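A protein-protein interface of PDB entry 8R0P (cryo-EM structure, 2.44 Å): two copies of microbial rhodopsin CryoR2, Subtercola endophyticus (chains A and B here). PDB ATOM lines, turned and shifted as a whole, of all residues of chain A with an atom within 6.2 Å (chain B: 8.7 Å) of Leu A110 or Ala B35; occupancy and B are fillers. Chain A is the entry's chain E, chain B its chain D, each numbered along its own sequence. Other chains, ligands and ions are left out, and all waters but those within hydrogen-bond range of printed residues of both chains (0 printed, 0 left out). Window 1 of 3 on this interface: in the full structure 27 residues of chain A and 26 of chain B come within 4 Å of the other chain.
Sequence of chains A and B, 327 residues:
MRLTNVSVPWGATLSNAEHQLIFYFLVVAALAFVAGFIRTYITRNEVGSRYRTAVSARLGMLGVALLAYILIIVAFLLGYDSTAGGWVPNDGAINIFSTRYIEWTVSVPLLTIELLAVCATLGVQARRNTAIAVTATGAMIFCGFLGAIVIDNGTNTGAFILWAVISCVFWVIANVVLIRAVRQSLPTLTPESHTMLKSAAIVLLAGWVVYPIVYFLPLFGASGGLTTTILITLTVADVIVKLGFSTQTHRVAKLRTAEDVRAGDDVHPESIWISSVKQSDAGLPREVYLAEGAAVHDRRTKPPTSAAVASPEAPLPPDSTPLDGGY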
ATOM      1  N   SER A  56      28.700   3.808 -20.904  1.00  0.00           N
ATOM      2  CA  SER A  56      27.844   2.787 -20.331  1.00  0.00           C
ATOM      3  C   SER A  56      28.598   1.464 -20.341  1.00  0.00           C
ATOM      4  O   SER A  56      28.527   0.708 -19.373  1.00  0.00           O
ATOM      5  CB  SER A  56      26.512   2.690 -21.028  1.00  0.00           C
ATOM      6  OG  SER A  56      26.669   2.252 -22.365  1.00  0.00           O
ATOM      7  N   ALA A  57      29.323   1.199 -21.429  1.00  0.00           N
ATOM      8  CA  ALA A  57      30.064  -0.036 -21.510  1.00  0.00           C
ATOM      9  C   ALA A  57      30.984  -0.103 -20.303  1.00  0.00           C
ATOM     10  O   ALA A  57      30.921  -1.089 -19.566  1.00  0.00           O
ATOM     11  CB  ALA A  57      30.820  -0.132 -22.802  1.00  0.00           C
ATOM     12  N   ARG A  58      31.760   0.972 -20.077  1.00  0.00           N
ATOM     13  CA  ARG A  58      32.775   0.999 -19.036  1.00  0.00           C
ATOM     14  C   ARG A  58      32.153   0.861 -17.657  1.00  0.00           C
ATOM     15  O   ARG A  58      32.653   0.151 -16.801  1.00  0.00           O
ATOM     16  CB  ARG A  58      33.585   2.290 -19.086  1.00  0.00           C
ATOM     17  CG  ARG A  58      34.713   2.404 -18.068  1.00  0.00           C
ATOM     18  CD  ARG A  58      35.633   1.187 -17.989  1.00  0.00           C
ATOM     19  NE  ARG A  58      36.415   0.973 -19.197  1.00  0.00           N
ATOM     20  CZ  ARG A  58      37.532   0.250 -19.277  1.00  0.00           C
ATOM     21  NH1 ARG A  58      38.077  -0.271 -18.198  1.00  0.00           N
ATOM     22  NH2 ARG A  58      38.119   0.055 -20.446  1.00  0.00           N
ATOM     23  N   GLY A  60      29.475  -0.558 -17.041  1.00  0.00           N
ATOM     24  CA  GLY A  60      28.977  -1.917 -17.011  1.00  0.00           C
ATOM     25  C   GLY A  60      30.114  -2.866 -16.688  1.00  0.00           C
ATOM     26  O   GLY A  60      30.036  -3.664 -15.756  1.00  0.00           O
ATOM     27  N   MET A  61      31.206  -2.705 -17.413  1.00  0.00           N
ATOM     28  CA  MET A  61      32.332  -3.565 -17.161  1.00  0.00           C
ATOM     29  C   MET A  61      32.776  -3.463 -15.694  1.00  0.00           C
ATOM     30  O   MET A  61      33.087  -4.475 -15.084  1.00  0.00           O
ATOM     31  CB  MET A  61      33.439  -3.248 -18.152  1.00  0.00           C
ATOM     32  CG  MET A  61      34.780  -3.801 -17.786  1.00  0.00           C
ATOM     33  SD  MET A  61      36.111  -3.016 -18.763  1.00  0.00           S
ATOM     34  CE  MET A  61      35.291  -2.646 -20.325  1.00  0.00           C
ATOM     35  N   LEU A  62      32.735  -2.281 -15.080  1.00  0.00           N
ATOM     36  CA  LEU A  62      33.254  -2.142 -13.727  1.00  0.00           C
ATOM     37  C   LEU A  62      32.281  -2.754 -12.741  1.00  0.00           C
ATOM     38  O   LEU A  62      32.713  -3.291 -11.731  1.00  0.00           O
ATOM     39  CB  LEU A  62      33.529  -0.676 -13.382  1.00  0.00           C
ATOM     40  CG  LEU A  62      34.808  -0.136 -14.016  1.00  0.00           C
ATOM     41  CD1 LEU A  62      34.791   1.376 -14.111  1.00  0.00           C
ATOM     42  CD2 LEU A  62      36.024  -0.613 -13.258  1.00  0.00           C
ATOM     43  N   VAL A  64      30.317  -5.305 -13.431  1.00  0.00           N
ATOM     44  CA  VAL A  64      30.447  -6.735 -13.610  1.00  0.00           C
ATOM     45  C   VAL A  64      31.674  -7.205 -12.838  1.00  0.00           C
ATOM     46  O   VAL A  64      31.621  -8.217 -12.152  1.00  0.00           O
ATOM     47  CB  VAL A  64      30.533  -7.088 -15.106  1.00  0.00           C
ATOM     48  CG1 VAL A  64      31.088  -8.474 -15.355  1.00  0.00           C
ATOM     49  CG2 VAL A  64      29.192  -6.930 -15.778  1.00  0.00           C
ATOM     50  N   THR A 105      33.636 -13.268 -19.657  1.00  0.00           N
ATOM     51  CA  THR A 105      32.738 -13.547 -20.749  1.00  0.00           C
ATOM     52  C   THR A 105      31.884 -12.302 -20.965  1.00  0.00           C
ATOM     53  O   THR A 105      31.535 -11.980 -22.099  1.00  0.00           O
ATOM     54  CB  THR A 105      31.924 -14.812 -20.484  1.00  0.00           C
ATOM     55  OG1 THR A 105      32.846 -15.811 -20.073  1.00  0.00           O
ATOM     56  CG2 THR A 105      31.182 -15.236 -21.723  1.00  0.00           C
ATOM     57  N   VAL A 106      31.555 -11.616 -19.873  1.00  0.00           N
ATOM     58  CA  VAL A 106      30.816 -10.390 -20.031  1.00  0.00           C
ATOM     59  C   VAL A 106      31.780  -9.245 -20.301  1.00  0.00           C
ATOM     60  O   VAL A 106      31.582  -8.495 -21.257  1.00  0.00           O
ATOM     61  CB  VAL A 106      29.898 -10.153 -18.834  1.00  0.00           C
ATOM     62  CG1 VAL A 106      29.140  -8.831 -18.939  1.00  0.00           C
ATOM     63  CG2 VAL A 106      28.941 -11.336 -18.719  1.00  0.00           C
ATOM     64  N   SER A 107      32.852  -9.165 -19.513  1.00  0.00           N
ATOM     65  CA  SER A 107      33.686  -7.975 -19.474  1.00  0.00           C
ATOM     66  C   SER A 107      34.433  -7.781 -20.785  1.00  0.00           C
ATOM     67  O   SER A 107      34.568  -6.663 -21.258  1.00  0.00           O
ATOM     68  CB  SER A 107      34.629  -8.006 -18.304  1.00  0.00           C
ATOM     69  OG  SER A 107      35.701  -8.905 -18.557  1.00  0.00           O
ATOM     70  N   VAL A 108      34.935  -8.829 -21.390  1.00  0.00           N
ATOM     71  CA  VAL A 108      35.740  -8.578 -22.563  1.00  0.00           C
ATOM     72  C   VAL A 108      34.871  -8.066 -23.706  1.00  0.00           C
ATOM     73  O   VAL A 108      35.288  -7.200 -24.462  1.00  0.00           O
ATOM     74  CB  VAL A 108      36.574  -9.807 -22.962  1.00  0.00           C
ATOM     75  CG1 VAL A 108      37.409  -9.551 -24.199  1.00  0.00           C
ATOM     76  CG2 VAL A 108      37.454 -10.229 -21.805  1.00  0.00           C
ATOM     77  N   PRO A 109      33.668  -8.600 -23.968  1.00  0.00           N
ATOM     78  CA  PRO A 109      32.804  -8.008 -24.999  1.00  0.00           C
ATOM     79  C   PRO A 109      32.438  -6.549 -24.699  1.00  0.00           C
ATOM     80  O   PRO A 109      32.391  -5.742 -25.615  1.00  0.00           O
ATOM     81  CB  PRO A 109      31.583  -8.943 -24.967  1.00  0.00           C
ATOM     82  CG  PRO A 109      32.178 -10.232 -24.517  1.00  0.00           C
ATOM     83  CD  PRO A 109      33.097  -9.821 -23.389  1.00  0.00           C
ATOM     84  N   LEU A 110      32.212  -6.218 -23.423  1.00  0.00           N
ATOM     85  CA  LEU A 110      32.039  -4.834 -23.024  1.00  0.00           C
ATOM     86  C   LEU A 110      33.235  -3.976 -23.436  1.00  0.00           C
ATOM     87  O   LEU A 110      33.052  -2.893 -23.973  1.00  0.00           O
ATOM     88  CB  LEU A 110      31.764  -4.752 -21.530  1.00  0.00           C
ATOM     89  CG  LEU A 110      30.334  -5.133 -21.138  1.00  0.00           C
ATOM     90  CD1 LEU A 110      30.116  -5.055 -19.635  1.00  0.00           C
ATOM     91  CD2 LEU A 110      29.328  -4.236 -21.846  1.00  0.00           C
ATOM     92  N   LEU A 111      34.451  -4.484 -23.293  1.00  0.00           N
ATOM     93  CA  LEU A 111      35.625  -3.738 -23.699  1.00  0.00           C
ATOM     94  C   LEU A 111      35.551  -3.479 -25.193  1.00  0.00           C
ATOM     95  O   LEU A 111      35.781  -2.374 -25.633  1.00  0.00           O
ATOM     96  CB  LEU A 111      36.858  -4.540 -23.304  1.00  0.00           C
ATOM     97  CG  LEU A 111      38.214  -3.852 -23.438  1.00  0.00           C
ATOM     98  CD1 LEU A 111      39.332  -4.792 -23.005  1.00  0.00           C
ATOM     99  CD2 LEU A 111      38.503  -3.385 -24.857  1.00  0.00           C
ATOM    100  N   THR A 112      35.169  -4.457 -25.995  1.00  0.00           N
ATOM    101  CA  THR A 112      35.135  -4.212 -27.427  1.00  0.00           C
ATOM    102  C   THR A 112      34.074  -3.153 -27.736  1.00  0.00           C
ATOM    103  O   THR A 112      34.274  -2.319 -28.613  1.00  0.00           O
ATOM    104  CB  THR A 112      34.903  -5.508 -28.225  1.00  0.00           C
ATOM    105  OG1 THR A 112      33.609  -6.037 -27.956  1.00  0.00           O
ATOM    106  CG2 THR A 112      35.909  -6.582 -27.892  1.00  0.00           C
ATOM    107  N   ILE A 113      32.939  -3.211 -27.037  1.00  0.00           N
ATOM    108  CA  ILE A 113      31.872  -2.263 -27.273  1.00  0.00           C
ATOM    109  C   ILE A 113      32.364  -0.846 -26.995  1.00  0.00           C
ATOM    110  O   ILE A 113      32.109   0.059 -27.785  1.00  0.00           O
ATOM    111  CB  ILE A 113      30.648  -2.597 -26.412  1.00  0.00           C
ATOM    112  CG1 ILE A 113      29.905  -3.799 -26.980  1.00  0.00           C
ATOM    113  CG2 ILE A 113      29.722  -1.408 -26.264  1.00  0.00           C
ATOM    114  CD1 ILE A 113      29.007  -4.404 -25.946  1.00  0.00           C
ATOM    115  N   GLU A 114      33.050  -0.682 -25.867  1.00  0.00           N
ATOM    116  CA  GLU A 114      33.632   0.583 -25.473  1.00  0.00           C
ATOM    117  C   GLU A 114      34.585   1.136 -26.526  1.00  0.00           C
ATOM    118  O   GLU A 114      34.511   2.309 -26.880  1.00  0.00           O
ATOM    119  CB  GLU A 114      34.410   0.402 -24.189  1.00  0.00           C
ATOM    120  CG  GLU A 114      34.779   1.699 -23.555  1.00  0.00           C
ATOM    121  CD  GLU A 114      35.294   1.543 -22.132  1.00  0.00           C
ATOM    122  OE1 GLU A 114      35.665   2.584 -21.522  1.00  0.00           O
ATOM    123  OE2 GLU A 114      35.310   0.394 -21.615  1.00  0.00           O
ATOM    124  N   LEU A 115      35.511   0.318 -27.001  1.00  0.00           N
ATOM    125  CA  LEU A 115      36.496   0.839 -27.921  1.00  0.00           C
ATOM    126  C   LEU A 115      35.834   1.203 -29.246  1.00  0.00           C
ATOM    127  O   LEU A 115      36.194   2.212 -29.847  1.00  0.00           O
ATOM    128  CB  LEU A 115      37.628  -0.173 -28.112  1.00  0.00           C
ATOM    129  CG  LEU A 115      38.718   0.254 -29.093  1.00  0.00           C
ATOM    130  CD1 LEU A 115      39.407   1.543 -28.645  1.00  0.00           C
ATOM    131  CD2 LEU A 115      39.742  -0.854 -29.249  1.00  0.00           C
ATOM    132  N   VAL A 134      31.925  -8.756 -30.479  1.00  0.00           N
ATOM    133  CA  VAL A 134      31.282  -9.267 -29.282  1.00  0.00           C
ATOM    134  C   VAL A 134      31.162 -10.781 -29.354  1.00  0.00           C
ATOM    135  O   VAL A 134      31.129 -11.461 -28.332  1.00  0.00           O
ATOM    136  CB  VAL A 134      29.912  -8.616 -29.066  1.00  0.00           C
ATOM    137  CG1 VAL A 134      29.089  -9.365 -28.029  1.00  0.00           C
ATOM    138  CG2 VAL A 134      30.080  -7.151 -28.662  1.00  0.00           C
ATOM    139  N   THR A 137      34.852 -12.408 -29.114  1.00  0.00           N
ATOM    140  CA  THR A 137      35.485 -12.339 -27.819  1.00  0.00           C
ATOM    141  C   THR A 137      34.775 -13.264 -26.847  1.00  0.00           C
ATOM    142  O   THR A 137      35.436 -13.829 -25.990  1.00  0.00           O
ATOM    143  CB  THR A 137      35.641 -10.910 -27.272  1.00  0.00           C
ATOM    144  OG1 THR A 137      34.374 -10.261 -27.153  1.00  0.00           O
ATOM    145  CG2 THR A 137      36.592 -10.112 -28.132  1.00  0.00           C
ATOM    146  N   VAL B  28      26.932 -15.967 -15.986  1.00  0.00           N
ATOM    147  CA  VAL B  28      27.055 -15.086 -17.113  1.00  0.00           C
ATOM    148  C   VAL B  28      25.760 -14.318 -17.362  1.00  0.00           C
ATOM    149  O   VAL B  28      25.824 -13.145 -17.716  1.00  0.00           O
ATOM    150  CB  VAL B  28      27.496 -15.844 -18.358  1.00  0.00           C
ATOM    151  CG1 VAL B  28      27.372 -14.986 -19.592  1.00  0.00           C
ATOM    152  CG2 VAL B  28      28.932 -16.320 -18.197  1.00  0.00           C
ATOM    153  N   ALA B  29      24.596 -14.952 -17.200  1.00  0.00           N
ATOM    154  CA  ALA B  29      23.333 -14.262 -17.405  1.00  0.00           C
ATOM    155  C   ALA B  29      23.185 -13.157 -16.374  1.00  0.00           C
ATOM    156  O   ALA B  29      22.949 -12.003 -16.732  1.00  0.00           O
ATOM    157  CB  ALA B  29      22.174 -15.199 -17.330  1.00  0.00           C
ATOM    158  N   ALA B  30      23.337 -13.509 -15.106  1.00  0.00           N
ATOM    159  CA  ALA B  30      23.182 -12.510 -14.066  1.00  0.00           C
ATOM    160  C   ALA B  30      24.085 -11.301 -14.319  1.00  0.00           C
ATOM    161  O   ALA B  30      23.696 -10.168 -14.060  1.00  0.00           O
ATOM    162  CB  ALA B  30      23.477 -13.099 -12.723  1.00  0.00           C
ATOM    163  N   LEU B  31      25.302 -11.541 -14.792  1.00  0.00           N
ATOM    164  CA  LEU B  31      26.249 -10.458 -14.969  1.00  0.00           C
ATOM    165  C   LEU B  31      25.885  -9.649 -16.208  1.00  0.00           C
ATOM    166  O   LEU B  31      25.938  -8.426 -16.179  1.00  0.00           O
ATOM    167  CB  LEU B  31      27.662 -11.039 -15.094  1.00  0.00           C
ATOM    168  CG  LEU B  31      28.276 -11.554 -13.786  1.00  0.00           C
ATOM    169  CD1 LEU B  31      29.714 -11.917 -14.035  1.00  0.00           C
ATOM    170  CD2 LEU B  31      28.193 -10.556 -12.647  1.00  0.00           C
ATOM    171  N   ALA B  32      25.510 -10.325 -17.291  1.00  0.00           N
ATOM    172  CA  ALA B  32      24.967  -9.606 -18.426  1.00  0.00           C
ATOM    173  C   ALA B  32      23.778  -8.726 -18.012  1.00  0.00           C
ATOM    174  O   ALA B  32      23.647  -7.606 -18.491  1.00  0.00           O
ATOM    175  CB  ALA B  32      24.600 -10.570 -19.508  1.00  0.00           C
ATOM    176  N   PHE B  33      22.910  -9.193 -17.116  1.00  0.00           N
ATOM    177  CA  PHE B  33      21.775  -8.367 -16.756  1.00  0.00           C
ATOM    178  C   PHE B  33      22.241  -7.162 -15.960  1.00  0.00           C
ATOM    179  O   PHE B  33      21.585  -6.130 -16.006  1.00  0.00           O
ATOM    180  CB  PHE B  33      20.671  -9.102 -15.980  1.00  0.00           C
ATOM    181  CG  PHE B  33      19.985 -10.159 -16.796  1.00  0.00           C
ATOM    182  CD1 PHE B  33      19.538  -9.875 -18.074  1.00  0.00           C
ATOM    183  CD2 PHE B  33      19.847 -11.459 -16.313  1.00  0.00           C
ATOM    184  CE1 PHE B  33      18.940 -10.859 -18.849  1.00  0.00           C
ATOM    185  CE2 PHE B  33      19.268 -12.448 -17.099  1.00  0.00           C
ATOM    186  CZ  PHE B  33      18.812 -12.143 -18.369  1.00  0.00           C
ATOM    187  N   VAL B  34      23.305  -7.292 -15.188  1.00  0.00           N
ATOM    188  CA  VAL B  34      23.765  -6.155 -14.410  1.00  0.00           C
ATOM    189  C   VAL B  34      24.281  -5.093 -15.376  1.00  0.00           C
ATOM    190  O   VAL B  34      23.979  -3.913 -15.251  1.00  0.00           O
ATOM    191  CB  VAL B  34      24.855  -6.555 -13.398  1.00  0.00           C
ATOM    192  CG1 VAL B  34      25.611  -5.348 -12.876  1.00  0.00           C
ATOM    193  CG2 VAL B  34      24.246  -7.336 -12.250  1.00  0.00           C
ATOM    194  N   ALA B  35      25.049  -5.540 -16.348  1.00  0.00           N
ATOM    195  CA  ALA B  35      25.502  -4.643 -17.364  1.00  0.00           C
ATOM    196  C   ALA B  35      24.299  -3.988 -18.042  1.00  0.00           C
ATOM    197  O   ALA B  35      24.280  -2.777 -18.204  1.00  0.00           O
ATOM    198  CB  ALA B  35      26.410  -5.357 -18.339  1.00  0.00           C
ATOM    199  N   GLY B  36      23.308  -4.762 -18.460  1.00  0.00           N
ATOM    200  CA  GLY B  36      22.145  -4.199 -19.131  1.00  0.00           C
ATOM    201  C   GLY B  36      21.406  -3.196 -18.255  1.00  0.00           C
ATOM    202  O   GLY B  36      20.960  -2.151 -18.716  1.00  0.00           O
ATOM    203  N   PHE B  37      21.290  -3.519 -16.983  1.00  0.00           N
ATOM    204  CA  PHE B  37      20.606  -2.617 -16.092  1.00  0.00           C
ATOM    205  C   PHE B  37      21.354  -1.291 -16.044  1.00  0.00           C
ATOM    206  O   PHE B  37      20.739  -0.236 -16.063  1.00  0.00           O
ATOM    207  CB  PHE B  37      20.426  -3.263 -14.724  1.00  0.00           C
ATOM    208  CG  PHE B  37      19.595  -2.451 -13.783  1.00  0.00           C
ATOM    209  CD1 PHE B  37      20.181  -1.452 -13.025  1.00  0.00           C
ATOM    210  CD2 PHE B  37      18.231  -2.671 -13.664  1.00  0.00           C
ATOM    211  CE1 PHE B  37      19.412  -0.694 -12.151  1.00  0.00           C
ATOM    212  CE2 PHE B  37      17.464  -1.925 -12.773  1.00  0.00           C
ATOM    213  CZ  PHE B  37      18.057  -0.935 -12.024  1.00  0.00           C
ATOM    214  N   ILE B  38      22.678  -1.337 -16.003  1.00  0.00           N
ATOM    215  CA  ILE B  38      23.447  -0.118 -15.919  1.00  0.00           C
ATOM    216  C   ILE B  38      23.285   0.694 -17.201  1.00  0.00           C
ATOM    217  O   ILE B  38      23.121   1.908 -17.128  1.00  0.00           O
ATOM    218  CB  ILE B  38      24.905  -0.446 -15.584  1.00  0.00           C
ATOM    219  CG1 ILE B  38      24.993  -0.870 -14.119  1.00  0.00           C
ATOM    220  CG2 ILE B  38      25.849   0.722 -15.867  1.00  0.00           C
ATOM    221  CD1 ILE B  38      26.255  -1.634 -13.817  1.00  0.00           C
ATOM    222  N   ARG B  39      23.294   0.039 -18.350  1.00  0.00           N
ATOM    223  CA  ARG B  39      23.178   0.743 -19.606  1.00  0.00           C
ATOM    224  C   ARG B  39      21.843   1.482 -19.654  1.00  0.00           C
ATOM    225  O   ARG B  39      21.783   2.683 -19.938  1.00  0.00           O
ATOM    226  CB  ARG B  39      23.253  -0.243 -20.764  1.00  0.00           C
ATOM    227  CG  ARG B  39      23.429   0.432 -22.099  1.00  0.00           C
ATOM    228  CD  ARG B  39      22.453  -0.025 -23.140  1.00  0.00           C
ATOM    229  NE  ARG B  39      22.418  -1.465 -23.389  1.00  0.00           N
ATOM    230  CZ  ARG B  39      21.456  -2.312 -22.980  1.00  0.00           C
ATOM    231  NH1 ARG B  39      20.623  -2.022 -21.983  1.00  0.00           N
ATOM    232  NH2 ARG B  39      21.389  -3.508 -23.544  1.00  0.00           N
ATOM    233  N   THR B  40      20.776   0.750 -19.314  1.00  0.00           N
ATOM    234  CA  THR B  40      19.433   1.263 -19.445  1.00  0.00           C
ATOM    235  C   THR B  40      19.248   2.445 -18.512  1.00  0.00           C
ATOM    236  O   THR B  40      18.585   3.411 -18.887  1.00  0.00           O
ATOM    237  CB  THR B  40      18.420   0.144 -19.251  1.00  0.00           C
ATOM    238  OG1 THR B  40      18.733  -0.759 -20.312  1.00  0.00           O
ATOM    239  CG2 THR B  40      16.980   0.603 -19.342  1.00  0.00           C
ATOM    240  N   TYR B  41      19.880   2.394 -17.345  1.00  0.00           N
ATOM    241  CA  TYR B  41      19.750   3.473 -16.388  1.00  0.00           C
ATOM    242  C   TYR B  41      20.491   4.708 -16.895  1.00  0.00           C
ATOM    243  O   TYR B  41      19.948   5.797 -16.885  1.00  0.00           O
ATOM    244  CB  TYR B  41      20.235   3.034 -15.007  1.00  0.00           C
ATOM    245  CG  TYR B  41      19.992   4.109 -13.969  1.00  0.00           C
ATOM    246  CD1 TYR B  41      18.715   4.345 -13.474  1.00  0.00           C
ATOM    247  CD2 TYR B  41      21.017   4.951 -13.561  1.00  0.00           C
ATOM    248  CE1 TYR B  41      18.470   5.365 -12.569  1.00  0.00           C
ATOM    249  CE2 TYR B  41      20.786   5.968 -12.650  1.00  0.00           C
ATOM    250  CZ  TYR B  41      19.510   6.176 -12.155  1.00  0.00           C
ATOM    251  OH  TYR B  41      19.262   7.182 -11.267  1.00  0.00           O
ATOM    252  N   ILE B  42      21.723   4.527 -17.359  1.00  0.00           N
ATOM    253  CA  ILE B  42      22.573   5.600 -17.846  1.00  0.00           C
ATOM    254  C   ILE B  42      21.937   6.258 -19.062  1.00  0.00           C
ATOM    255  O   ILE B  42      22.179   7.428 -19.302  1.00  0.00           O
ATOM    256  CB  ILE B  42      24.000   5.045 -18.102  1.00  0.00           C
ATOM    257  CG1 ILE B  42      24.905   5.353 -16.923  1.00  0.00           C
ATOM    258  CG2 ILE B  42      24.672   5.528 -19.365  1.00  0.00           C
ATOM    259  CD1 ILE B  42      24.175   5.281 -15.598  1.00  0.00           C
ATOM    260  N   LEU B  59      13.711  -1.051 -17.775  1.00  0.00           N
ATOM    261  CA  LEU B  59      14.616  -1.023 -16.651  1.00  0.00           C
ATOM    262  C   LEU B  59      14.068  -1.921 -15.556  1.00  0.00           C
ATOM    263  O   LEU B  59      14.825  -2.501 -14.785  1.00  0.00           O
ATOM    264  CB  LEU B  59      14.781   0.421 -16.185  1.00  0.00           C
ATOM    265  CG  LEU B  59      15.859   0.637 -15.133  1.00  0.00           C
ATOM    266  CD1 LEU B  59      17.234   0.187 -15.611  1.00  0.00           C
ATOM    267  CD2 LEU B  59      15.892   2.109 -14.778  1.00  0.00           C
ATOM    268  N   LEU B  62      14.809  -5.522 -16.459  1.00  0.00           N
ATOM    269  CA  LEU B  62      16.199  -5.918 -16.288  1.00  0.00           C
ATOM    270  C   LEU B  62      16.507  -6.083 -14.815  1.00  0.00           C
ATOM    271  O   LEU B  62      17.312  -6.935 -14.464  1.00  0.00           O
ATOM    272  CB  LEU B  62      17.152  -4.908 -16.933  1.00  0.00           C
ATOM    273  CG  LEU B  62      17.218  -5.027 -18.454  1.00  0.00           C
ATOM    274  CD1 LEU B  62      17.713  -3.747 -19.095  1.00  0.00           C
ATOM    275  CD2 LEU B  62      18.077  -6.200 -18.863  1.00  0.00           C
ATOM    276  N   LEU B  66      17.659  -9.615 -13.073  1.00  0.00           N
ATOM    277  CA  LEU B  66      18.877  -9.666 -12.290  1.00  0.00           C
ATOM    278  C   LEU B  66      18.589 -10.323 -10.939  1.00  0.00           C
ATOM    279  O   LEU B  66      19.321 -11.211 -10.530  1.00  0.00           O
ATOM    280  CB  LEU B  66      19.403  -8.232 -12.165  1.00  0.00           C
ATOM    281  CG  LEU B  66      20.731  -8.034 -11.442  1.00  0.00           C
ATOM    282  CD1 LEU B  66      20.488  -7.693  -9.998  1.00  0.00           C
ATOM    283  CD2 LEU B  66      21.620  -9.271 -11.539  1.00  0.00           C
ATOM    284  N   LEU B 243      18.062  -8.961 -22.798  1.00  0.00           N
ATOM    285  CA  LEU B 243      19.220  -8.096 -22.932  1.00  0.00           C
ATOM    286  C   LEU B 243      19.380  -7.735 -24.400  1.00  0.00           C
ATOM    287  O   LEU B 243      19.306  -6.575 -24.776  1.00  0.00           O
ATOM    288  CB  LEU B 243      20.445  -8.834 -22.406  1.00  0.00           C
ATOM    289  CG  LEU B 243      21.427  -8.027 -21.580  1.00  0.00           C
ATOM    290  CD1 LEU B 243      22.820  -8.191 -22.160  1.00  0.00           C
ATOM    291  CD2 LEU B 243      21.036  -6.564 -21.481  1.00  0.00           C
ATOM    292  N   SER B 246      16.781  -5.385 -25.645  1.00  0.00           N
ATOM    293  CA  SER B 246      16.526  -4.285 -24.729  1.00  0.00           C
ATOM    294  C   SER B 246      16.722  -2.938 -25.412  1.00  0.00           C
ATOM    295  O   SER B 246      16.330  -1.922 -24.849  1.00  0.00           O
ATOM    296  CB  SER B 246      17.376  -4.366 -23.477  1.00  0.00           C
ATOM    297  OG  SER B 246      18.748  -4.254 -23.770  1.00  0.00           O
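Of the printed residues of chain B, Val A64 touches Leu B31. Printed residues of chain B within 4 Å of Val A106: Val B28 (3.7 Å), Leu B31 (3.9 Å) and Ala B32 (3.9 Å). Of chain B, only Ala B35 (3.9 Å) comes within 4 Å of Leu A110. Printed residues of chain A within 4 Å of Val B28: Val A106 (3.7 Å). Printed residues of chain A within 4 Å of Ala B32: Val A106 (3.9 Å). Ala B35 touches just one residue of chain A: Leu A110.
The backbone carbonyl oxygen (O) of Gly B36 is in hydrogen-bond range of the guanidinium group (NH1) of Arg B39 (3.3 Å). NH1 of Arg B39 sits at hydrogen-bond distance from OG1 of Thr B40 (2.8 Å). NH2 of Arg B39 is in hydrogen-bond range of OG of Ser B246.
Hydrophobic or aromatic side chains of chain B within 4 Å of the printed part of chain A: Leu B31, Ala B35 and Ile B42. Printed residues of chain A that touch a printed residue of chain B: Ser A56, Val A64, Val A106 and Leu A110. Among the printed residues, no Asp or Glu carboxylate lies within 4 Å of a Lys or Arg side-chain nitrogen of the other chain.
Among the printed residues, pairs that only touch across the chains: Val A64 with Leu B31 (3.6 Å), Ser A56 with Arg B39 (3.7 Å), Val A106 with Val B28 (3.7 Å), Ser A56 with Ile B42 (3.8 Å), Val A106 with Ala B32 (3.9 Å), Val A106 with Leu B31 (3.9 Å) and Leu A110 with Ala B35 (3.9 Å).
1 position is printed for both chains. Of the 7 pairs that touch across the chains among the printed residues, none has its exchanged pair printed and touching as well.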
